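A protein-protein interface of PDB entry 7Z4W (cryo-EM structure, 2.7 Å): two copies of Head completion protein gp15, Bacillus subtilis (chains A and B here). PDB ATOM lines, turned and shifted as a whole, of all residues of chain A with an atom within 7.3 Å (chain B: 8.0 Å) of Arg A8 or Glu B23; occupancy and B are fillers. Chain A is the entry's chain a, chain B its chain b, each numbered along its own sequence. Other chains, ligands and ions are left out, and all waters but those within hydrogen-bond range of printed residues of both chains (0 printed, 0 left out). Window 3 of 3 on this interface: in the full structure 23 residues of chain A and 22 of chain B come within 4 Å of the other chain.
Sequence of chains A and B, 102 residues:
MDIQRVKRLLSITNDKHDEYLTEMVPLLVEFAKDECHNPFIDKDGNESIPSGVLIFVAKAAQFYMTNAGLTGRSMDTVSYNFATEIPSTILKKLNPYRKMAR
Of chain B, only Glu B19, Tyr B20 and Glu B23 come within 4 Å of Arg A8. Glu B23 touches just these residues of chain A: Arg A5 and Arg A8. Of the printed residues of chain A, Glu B19 touches Arg A8 (3.4 Å). Printed residues of chain A within 4 Å of Met B24: Leu A9 (3.9 Å). Of the printed residues of chain B, Ser A11 touches Tyr B20 (3.9 Å). Printed residues of chain A within 4 Å of Tyr B20: Arg A8, Leu A9 and Ser A11. Pro B26 touches none of the printed residues of chain A. The nearest residue of chain B that does not touch Arg A8 is Leu B21 (6.2 Å). The nearest residue of chain A that does not touch Glu B23 is Leu A9 (4.2 Å). The nearest printed residue of chain B that does not touch Ser A11 is Glu B19 (5.9 Å).
Position printed for both chains: 3. Of the 9 pairs that touch across the chains among the printed residues, none has its exchanged pair printed and touching as well.
The side-chain carboxylate (OE1) of Glu B23 is in salt-bridge range of the guanidinium group (NE) of Arg A5 (3.3 Å). The side-chain carboxylate (OE2) of Glu B23 lies within salt-bridge range of the guanidinium group (NH2) of Arg A8 (3.7 Å).
Leu B27 touches Arg A5 (CD2 to NH2, 3.7 Å). Glu B19 touches Arg A8 (OE2 to CG, 3.4 Å). CA of Tyr B20 touches O of Arg A8 (3.9 Å). O of Leu A9 touches CD1 of Tyr B20 (3.6 Å). Leu A9 touches Met B24 (CD2 to CE, 3.9 Å). Leu B27 touches Leu A9. OG of Ser A11 touches CB of Tyr B20, 3.9 Å away.
Of the 13 printed residues of chain B, 5 touch a printed residue of chain A. Hydrophobic or aromatic side chains of chain B within 4 Å of the printed part of chain A: Tyr B20, Met B24 and Leu B27. Hydrophobic or aromatic side chains of chain A within 4 Å of the printed part of chain B: Leu A9. Among the printed residues, 9 pairs touch across the chains.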
ATOM      1  N   MET A   1      -5.692  -8.813  -2.557  1.00  0.00           N
ATOM      2  CA  MET A   1      -6.023  -9.023  -1.156  1.00  0.00           C
ATOM      3  C   MET A   1      -6.155  -7.692  -0.425  1.00  0.00           C
ATOM      4  O   MET A   1      -5.358  -6.779  -0.612  1.00  0.00           O
ATOM      5  CB  MET A   1      -4.969  -9.905  -0.484  1.00  0.00           C
ATOM      6  CG  MET A   1      -5.399 -10.498   0.845  1.00  0.00           C
ATOM      7  SD  MET A   1      -4.323 -11.833   1.407  1.00  0.00           S
ATOM      8  CE  MET A   1      -5.181 -12.370   2.885  1.00  0.00           C
ATOM      9  N   ASP A   2      -7.184  -7.603   0.407  1.00  0.00           N
ATOM     10  CA  ASP A   2      -7.453  -6.396   1.169  1.00  0.00           C
ATOM     11  C   ASP A   2      -6.446  -6.244   2.307  1.00  0.00           C
ATOM     12  O   ASP A   2      -6.090  -7.217   2.972  1.00  0.00           O
ATOM     13  CB  ASP A   2      -8.882  -6.460   1.702  1.00  0.00           C
ATOM     14  CG  ASP A   2      -9.272  -5.244   2.492  1.00  0.00           C
ATOM     15  OD1 ASP A   2      -8.775  -4.141   2.192  1.00  0.00           O
ATOM     16  OD2 ASP A   2     -10.099  -5.399   3.413  1.00  0.00           O
ATOM     17  N   ILE A   3      -5.987  -5.010   2.524  1.00  0.00           N
ATOM     18  CA  ILE A   3      -4.944  -4.748   3.515  1.00  0.00           C
ATOM     19  C   ILE A   3      -5.500  -4.868   4.933  1.00  0.00           C
ATOM     20  O   ILE A   3      -4.836  -5.404   5.832  1.00  0.00           O
ATOM     21  CB  ILE A   3      -4.307  -3.368   3.235  1.00  0.00           C
ATOM     22  CG1 ILE A   3      -3.421  -3.434   1.992  1.00  0.00           C
ATOM     23  CG2 ILE A   3      -3.481  -2.847   4.395  1.00  0.00           C
ATOM     24  CD1 ILE A   3      -2.372  -4.497   2.038  1.00  0.00           C
ATOM     25  N   GLN A   4      -6.740  -4.414   5.146  1.00  0.00           N
ATOM     26  CA  GLN A   4      -7.358  -4.510   6.464  1.00  0.00           C
ATOM     27  C   GLN A   4      -7.669  -5.953   6.847  1.00  0.00           C
ATOM     28  O   GLN A   4      -7.622  -6.300   8.031  1.00  0.00           O
ATOM     29  CB  GLN A   4      -8.624  -3.657   6.515  1.00  0.00           C
ATOM     30  CG  GLN A   4      -8.406  -2.201   6.155  1.00  0.00           C
ATOM     31  CD  GLN A   4      -7.444  -1.495   7.089  1.00  0.00           C
ATOM     32  OE1 GLN A   4      -7.478  -1.695   8.300  1.00  0.00           O
ATOM     33  NE2 GLN A   4      -6.581  -0.659   6.528  1.00  0.00           N
ATOM     34  N   ARG A   5      -7.938  -6.811   5.861  1.00  0.00           N
ATOM     35  CA  ARG A   5      -8.122  -8.234   6.130  1.00  0.00           C
ATOM     36  C   ARG A   5      -6.819  -8.895   6.579  1.00  0.00           C
ATOM     37  O   ARG A   5      -6.825  -9.734   7.489  1.00  0.00           O
ATOM     38  CB  ARG A   5      -8.681  -8.922   4.887  1.00  0.00           C
ATOM     39  CG  ARG A   5      -9.230 -10.303   5.137  1.00  0.00           C
ATOM     40  CD  ARG A   5      -9.704 -10.935   3.857  1.00  0.00           C
ATOM     41  NE  ARG A   5     -10.314 -12.238   4.083  1.00  0.00           N
ATOM     42  CZ  ARG A   5     -10.730 -13.043   3.115  1.00  0.00           C
ATOM     43  NH1 ARG A   5     -10.605 -12.680   1.851  1.00  0.00           N
ATOM     44  NH2 ARG A   5     -11.269 -14.213   3.412  1.00  0.00           N
ATOM     45  N   VAL A   6      -5.691  -8.510   5.971  1.00  0.00           N
ATOM     46  CA  VAL A   6      -4.385  -9.017   6.393  1.00  0.00           C
ATOM     47  C   VAL A   6      -4.042  -8.522   7.796  1.00  0.00           C
ATOM     48  O   VAL A   6      -3.504  -9.275   8.621  1.00  0.00           O
ATOM     49  CB  VAL A   6      -3.305  -8.615   5.366  1.00  0.00           C
ATOM     50  CG1 VAL A   6      -1.922  -9.069   5.804  1.00  0.00           C
ATOM     51  CG2 VAL A   6      -3.628  -9.180   4.004  1.00  0.00           C
ATOM     52  N   LYS A   7      -4.374  -7.260   8.095  1.00  0.00           N
ATOM     53  CA  LYS A   7      -4.150  -6.728   9.437  1.00  0.00           C
ATOM     54  C   LYS A   7      -5.011  -7.429  10.483  1.00  0.00           C
ATOM     55  O   LYS A   7      -4.566  -7.614  11.620  1.00  0.00           O
ATOM     56  CB  LYS A   7      -4.411  -5.225   9.463  1.00  0.00           C
ATOM     57  CG  LYS A   7      -3.226  -4.387   9.040  1.00  0.00           C
ATOM     58  CD  LYS A   7      -3.648  -2.980   8.704  1.00  0.00           C
ATOM     59  CE  LYS A   7      -4.023  -2.224   9.952  1.00  0.00           C
ATOM     60  NZ  LYS A   7      -4.241  -0.799   9.673  1.00  0.00           N
ATOM     61  N   ARG A   8      -6.230  -7.837  10.121  1.00  0.00           N
ATOM     62  CA  ARG A   8      -7.023  -8.649  11.038  1.00  0.00           C
ATOM     63  C   ARG A   8      -6.443 -10.052  11.196  1.00  0.00           C
ATOM     64  O   ARG A   8      -6.515 -10.628  12.285  1.00  0.00           O
ATOM     65  CB  ARG A   8      -8.476  -8.723  10.570  1.00  0.00           C
ATOM     66  CG  ARG A   8      -9.258  -7.437  10.760  1.00  0.00           C
ATOM     67  CD  ARG A   8     -10.751  -7.647  10.570  1.00  0.00           C
ATOM     68  NE  ARG A   8     -11.079  -8.101   9.223  1.00  0.00           N
ATOM     69  CZ  ARG A   8     -11.293  -7.298   8.188  1.00  0.00           C
ATOM     70  NH1 ARG A   8     -11.217  -5.984   8.335  1.00  0.00           N
ATOM     71  NH2 ARG A   8     -11.579  -7.811   7.004  1.00  0.00           N
ATOM     72  N   LEU A   9      -5.854 -10.610  10.134  1.00  0.00           N
ATOM     73  CA  LEU A   9      -5.265 -11.942  10.231  1.00  0.00           C
ATOM     74  C   LEU A   9      -3.944 -11.961  10.994  1.00  0.00           C
ATOM     75  O   LEU A   9      -3.542 -13.024  11.473  1.00  0.00           O
ATOM     76  CB  LEU A   9      -5.047 -12.535   8.837  1.00  0.00           C
ATOM     77  CG  LEU A   9      -6.232 -13.208   8.146  1.00  0.00           C
ATOM     78  CD1 LEU A   9      -5.971 -13.331   6.661  1.00  0.00           C
ATOM     79  CD2 LEU A   9      -6.515 -14.569   8.751  1.00  0.00           C
ATOM     80  N   LEU A  10      -3.256 -10.827  11.116  1.00  0.00           N
ATOM     81  CA  LEU A  10      -1.980 -10.780  11.821  1.00  0.00           C
ATOM     82  C   LEU A  10      -2.050 -10.090  13.178  1.00  0.00           C
ATOM     83  O   LEU A  10      -1.002  -9.920  13.812  1.00  0.00           O
ATOM     84  CB  LEU A  10      -0.913 -10.095  10.958  1.00  0.00           C
ATOM     85  CG  LEU A  10      -0.561 -10.727   9.608  1.00  0.00           C
ATOM     86  CD1 LEU A  10       0.508  -9.916   8.906  1.00  0.00           C
ATOM     87  CD2 LEU A  10      -0.118 -12.174   9.768  1.00  0.00           C
ATOM     88  N   SER A  11      -3.250  -9.694  13.629  1.00  0.00           N
ATOM     89  CA  SER A  11      -3.498  -9.013  14.912  1.00  0.00           C
ATOM     90  C   SER A  11      -2.718  -7.701  15.037  1.00  0.00           C
ATOM     91  O   SER A  11      -2.072  -7.432  16.049  1.00  0.00           O
ATOM     92  CB  SER A  11      -3.211  -9.934  16.104  1.00  0.00           C
ATOM     93  OG  SER A  11      -4.054 -11.068  16.101  1.00  0.00           O
ATOM     94  N   ILE A  12      -2.802  -6.874  14.002  1.00  0.00           N
ATOM     95  CA  ILE A  12      -2.203  -5.544  13.995  1.00  0.00           C
ATOM     96  C   ILE A  12      -3.317  -4.521  14.167  1.00  0.00           C
ATOM     97  O   ILE A  12      -4.333  -4.578  13.464  1.00  0.00           O
ATOM     98  CB  ILE A  12      -1.415  -5.298  12.696  1.00  0.00           C
ATOM     99  CG1 ILE A  12      -0.275  -6.308  12.568  1.00  0.00           C
ATOM    100  CG2 ILE A  12      -0.868  -3.890  12.639  1.00  0.00           C
ATOM    101  CD1 ILE A  12       0.440  -6.253  11.243  1.00  0.00           C
ATOM    102  N   THR A  13      -3.139  -3.590  15.105  1.00  0.00           N
ATOM    103  CA  THR A  13      -4.151  -2.576  15.377  1.00  0.00           C
ATOM    104  C   THR A  13      -3.761  -1.164  14.966  1.00  0.00           C
ATOM    105  O   THR A  13      -4.642  -0.394  14.589  1.00  0.00           O
ATOM    106  CB  THR A  13      -4.519  -2.567  16.866  1.00  0.00           C
ATOM    107  OG1 THR A  13      -3.348  -2.323  17.653  1.00  0.00           O
ATOM    108  CG2 THR A  13      -5.142  -3.888  17.272  1.00  0.00           C
ATOM    109  N   ILE B   3     -17.368 -20.178  16.507  1.00  0.00           N
ATOM    110  CA  ILE B   3     -16.228 -19.526  17.147  1.00  0.00           C
ATOM    111  C   ILE B   3     -16.209 -19.808  18.651  1.00  0.00           C
ATOM    112  O   ILE B   3     -15.141 -20.014  19.245  1.00  0.00           O
ATOM    113  CB  ILE B   3     -16.264 -18.018  16.826  1.00  0.00           C
ATOM    114  CG1 ILE B   3     -16.015 -17.794  15.335  1.00  0.00           C
ATOM    115  CG2 ILE B   3     -15.248 -17.225  17.617  1.00  0.00           C
ATOM    116  CD1 ILE B   3     -14.703 -18.325  14.839  1.00  0.00           C
ATOM    117  N   HIS B  17      -9.204 -12.463  21.525  1.00  0.00           N
ATOM    118  CA  HIS B  17      -8.837 -13.111  20.275  1.00  0.00           C
ATOM    119  C   HIS B  17      -9.989 -13.206  19.280  1.00  0.00           C
ATOM    120  O   HIS B  17      -9.880 -13.964  18.316  1.00  0.00           O
ATOM    121  CB  HIS B  17      -8.301 -14.520  20.533  1.00  0.00           C
ATOM    122  CG  HIS B  17      -7.405 -14.636  21.725  1.00  0.00           C
ATOM    123  ND1 HIS B  17      -7.878 -14.943  22.982  1.00  0.00           N
ATOM    124  CD2 HIS B  17      -6.061 -14.526  21.846  1.00  0.00           C
ATOM    125  CE1 HIS B  17      -6.868 -15.000  23.831  1.00  0.00           C
ATOM    126  NE2 HIS B  17      -5.754 -14.749  23.167  1.00  0.00           N
ATOM    127  N   ASP B  18     -11.076 -12.454  19.479  1.00  0.00           N
ATOM    128  CA  ASP B  18     -12.306 -12.705  18.726  1.00  0.00           C
ATOM    129  C   ASP B  18     -12.184 -12.273  17.268  1.00  0.00           C
ATOM    130  O   ASP B  18     -12.654 -12.978  16.363  1.00  0.00           O
ATOM    131  CB  ASP B  18     -13.482 -11.989  19.385  1.00  0.00           C
ATOM    132  CG  ASP B  18     -14.163 -12.830  20.444  1.00  0.00           C
ATOM    133  OD1 ASP B  18     -13.551 -13.791  20.946  1.00  0.00           O
ATOM    134  OD2 ASP B  18     -15.322 -12.525  20.780  1.00  0.00           O
ATOM    135  N   GLU B  19     -11.542 -11.131  17.025  1.00  0.00           N
ATOM    136  CA  GLU B  19     -11.424 -10.603  15.673  1.00  0.00           C
ATOM    137  C   GLU B  19     -10.470 -11.440  14.824  1.00  0.00           C
ATOM    138  O   GLU B  19     -10.692 -11.597  13.619  1.00  0.00           O
ATOM    139  CB  GLU B  19     -10.986  -9.140  15.748  1.00  0.00           C
ATOM    140  CG  GLU B  19     -10.753  -8.457  14.427  1.00  0.00           C
ATOM    141  CD  GLU B  19     -10.073  -7.117  14.582  1.00  0.00           C
ATOM    142  OE1 GLU B  19     -10.664  -6.224  15.225  1.00  0.00           O
ATOM    143  OE2 GLU B  19      -8.950  -6.950  14.065  1.00  0.00           O
ATOM    144  N   TYR B  20      -9.432 -12.012  15.440  1.00  0.00           N
ATOM    145  CA  TYR B  20      -8.540 -12.922  14.726  1.00  0.00           C
ATOM    146  C   TYR B  20      -9.237 -14.237  14.389  1.00  0.00           C
ATOM    147  O   TYR B  20      -9.068 -14.766  13.284  1.00  0.00           O
ATOM    148  CB  TYR B  20      -7.278 -13.178  15.558  1.00  0.00           C
ATOM    149  CG  TYR B  20      -6.496 -14.417  15.160  1.00  0.00           C
ATOM    150  CD1 TYR B  20      -5.691 -14.420  14.030  1.00  0.00           C
ATOM    151  CD2 TYR B  20      -6.559 -15.582  15.921  1.00  0.00           C
ATOM    152  CE1 TYR B  20      -4.979 -15.546  13.662  1.00  0.00           C
ATOM    153  CE2 TYR B  20      -5.859 -16.711  15.554  1.00  0.00           C
ATOM    154  CZ  TYR B  20      -5.066 -16.686  14.429  1.00  0.00           C
ATOM    155  OH  TYR B  20      -4.363 -17.804  14.067  1.00  0.00           O
ATOM    156  N   LEU B  21     -10.019 -14.778  15.329  1.00  0.00           N
ATOM    157  CA  LEU B  21     -10.641 -16.084  15.129  1.00  0.00           C
ATOM    158  C   LEU B  21     -11.753 -16.021  14.090  1.00  0.00           C
ATOM    159  O   LEU B  21     -11.891 -16.944  13.271  1.00  0.00           O
ATOM    160  CB  LEU B  21     -11.179 -16.621  16.456  1.00  0.00           C
ATOM    161  CG  LEU B  21     -10.159 -17.165  17.459  1.00  0.00           C
ATOM    162  CD1 LEU B  21     -10.817 -17.413  18.805  1.00  0.00           C
ATOM    163  CD2 LEU B  21      -9.496 -18.428  16.946  1.00  0.00           C
ATOM    164  N   THR B  22     -12.521 -14.919  14.089  1.00  0.00           N
ATOM    165  CA  THR B  22     -13.590 -14.711  13.113  1.00  0.00           C
ATOM    166  C   THR B  22     -13.062 -14.666  11.680  1.00  0.00           C
ATOM    167  O   THR B  22     -13.767 -15.055  10.745  1.00  0.00           O
ATOM    168  CB  THR B  22     -14.338 -13.417  13.451  1.00  0.00           C
ATOM    169  OG1 THR B  22     -14.568 -13.359  14.860  1.00  0.00           O
ATOM    170  CG2 THR B  22     -15.672 -13.341  12.745  1.00  0.00           C
ATOM    171  N   GLU B  23     -11.821 -14.228  11.491  1.00  0.00           N
ATOM    172  CA  GLU B  23     -11.196 -14.240  10.177  1.00  0.00           C
ATOM    173  C   GLU B  23     -10.498 -15.559   9.860  1.00  0.00           C
ATOM    174  O   GLU B  23     -10.535 -16.010   8.713  1.00  0.00           O
ATOM    175  CB  GLU B  23     -10.194 -13.091  10.067  1.00  0.00           C
ATOM    176  CG  GLU B  23     -10.790 -11.807   9.549  1.00  0.00           C
ATOM    177  CD  GLU B  23     -11.188 -11.908   8.099  1.00  0.00           C
ATOM    178  OE1 GLU B  23     -10.432 -12.525   7.329  1.00  0.00           O
ATOM    179  OE2 GLU B  23     -12.253 -11.380   7.731  1.00  0.00           O
ATOM    180  N   MET B  24      -9.869 -16.193  10.852  1.00  0.00           N
ATOM    181  CA  MET B  24      -8.964 -17.310  10.597  1.00  0.00           C
ATOM    182  C   MET B  24      -9.669 -18.665  10.497  1.00  0.00           C
ATOM    183  O   MET B  24      -9.236 -19.515   9.713  1.00  0.00           O
ATOM    184  CB  MET B  24      -7.878 -17.339  11.684  1.00  0.00           C
ATOM    185  CG  MET B  24      -6.819 -18.434  11.559  1.00  0.00           C
ATOM    186  SD  MET B  24      -6.068 -18.588   9.922  1.00  0.00           S
ATOM    187  CE  MET B  24      -4.545 -17.680  10.136  1.00  0.00           C
ATOM    188  N   VAL B  25     -10.756 -18.883  11.255  1.00  0.00           N
ATOM    189  CA  VAL B  25     -11.404 -20.208  11.277  1.00  0.00           C
ATOM    190  C   VAL B  25     -12.021 -20.640   9.938  1.00  0.00           C
ATOM    191  O   VAL B  25     -11.765 -21.784   9.512  1.00  0.00           O
ATOM    192  CB  VAL B  25     -12.393 -20.283  12.457  1.00  0.00           C
ATOM    193  CG1 VAL B  25     -13.319 -21.483  12.354  1.00  0.00           C
ATOM    194  CG2 VAL B  25     -11.629 -20.315  13.773  1.00  0.00           C
ATOM    195  N   PRO B  26     -12.816 -19.807   9.218  1.00  0.00           N
ATOM    196  CA  PRO B  26     -13.363 -20.291   7.931  1.00  0.00           C
ATOM    197  C   PRO B  26     -12.315 -20.542   6.857  1.00  0.00           C
ATOM    198  O   PRO B  26     -12.504 -21.439   6.019  1.00  0.00           O
ATOM    199  CB  PRO B  26     -14.321 -19.170   7.510  1.00  0.00           C
ATOM    200  CG  PRO B  26     -14.610 -18.438   8.718  1.00  0.00           C
ATOM    201  CD  PRO B  26     -13.377 -18.466   9.506  1.00  0.00           C
ATOM    202  N   LEU B  27     -11.209 -19.792   6.885  1.00  0.00           N
ATOM    203  CA  LEU B  27     -10.100 -20.038   5.967  1.00  0.00           C
ATOM    204  C   LEU B  27      -9.472 -21.404   6.208  1.00  0.00           C
ATOM    205  O   LEU B  27      -9.116 -22.104   5.257  1.00  0.00           O
ATOM    206  CB  LEU B  27      -9.045 -18.942   6.114  1.00  0.00           C
ATOM    207  CG  LEU B  27      -9.381 -17.540   5.610  1.00  0.00           C
ATOM    208  CD1 LEU B  27      -8.200 -16.612   5.822  1.00  0.00           C
ATOM    209  CD2 LEU B  27      -9.785 -17.569   4.153  1.00  0.00           C
ATOM    210  N   LEU B  28      -9.353 -21.814   7.473  1.00  0.00           N
ATOM    211  CA  LEU B  28      -8.789 -23.124   7.777  1.00  0.00           C
ATOM    212  C   LEU B  28      -9.753 -24.252   7.431  1.00  0.00           C
ATOM    213  O   LEU B  28      -9.310 -25.345   7.049  1.00  0.00           O
ATOM    214  CB  LEU B  28      -8.388 -23.193   9.250  1.00  0.00           C
ATOM    215  CG  LEU B  28      -7.129 -22.408   9.623  1.00  0.00           C
ATOM    216  CD1 LEU B  28      -7.005 -22.272  11.131  1.00  0.00           C
ATOM    217  CD2 LEU B  28      -5.888 -23.056   9.036  1.00  0.00           C
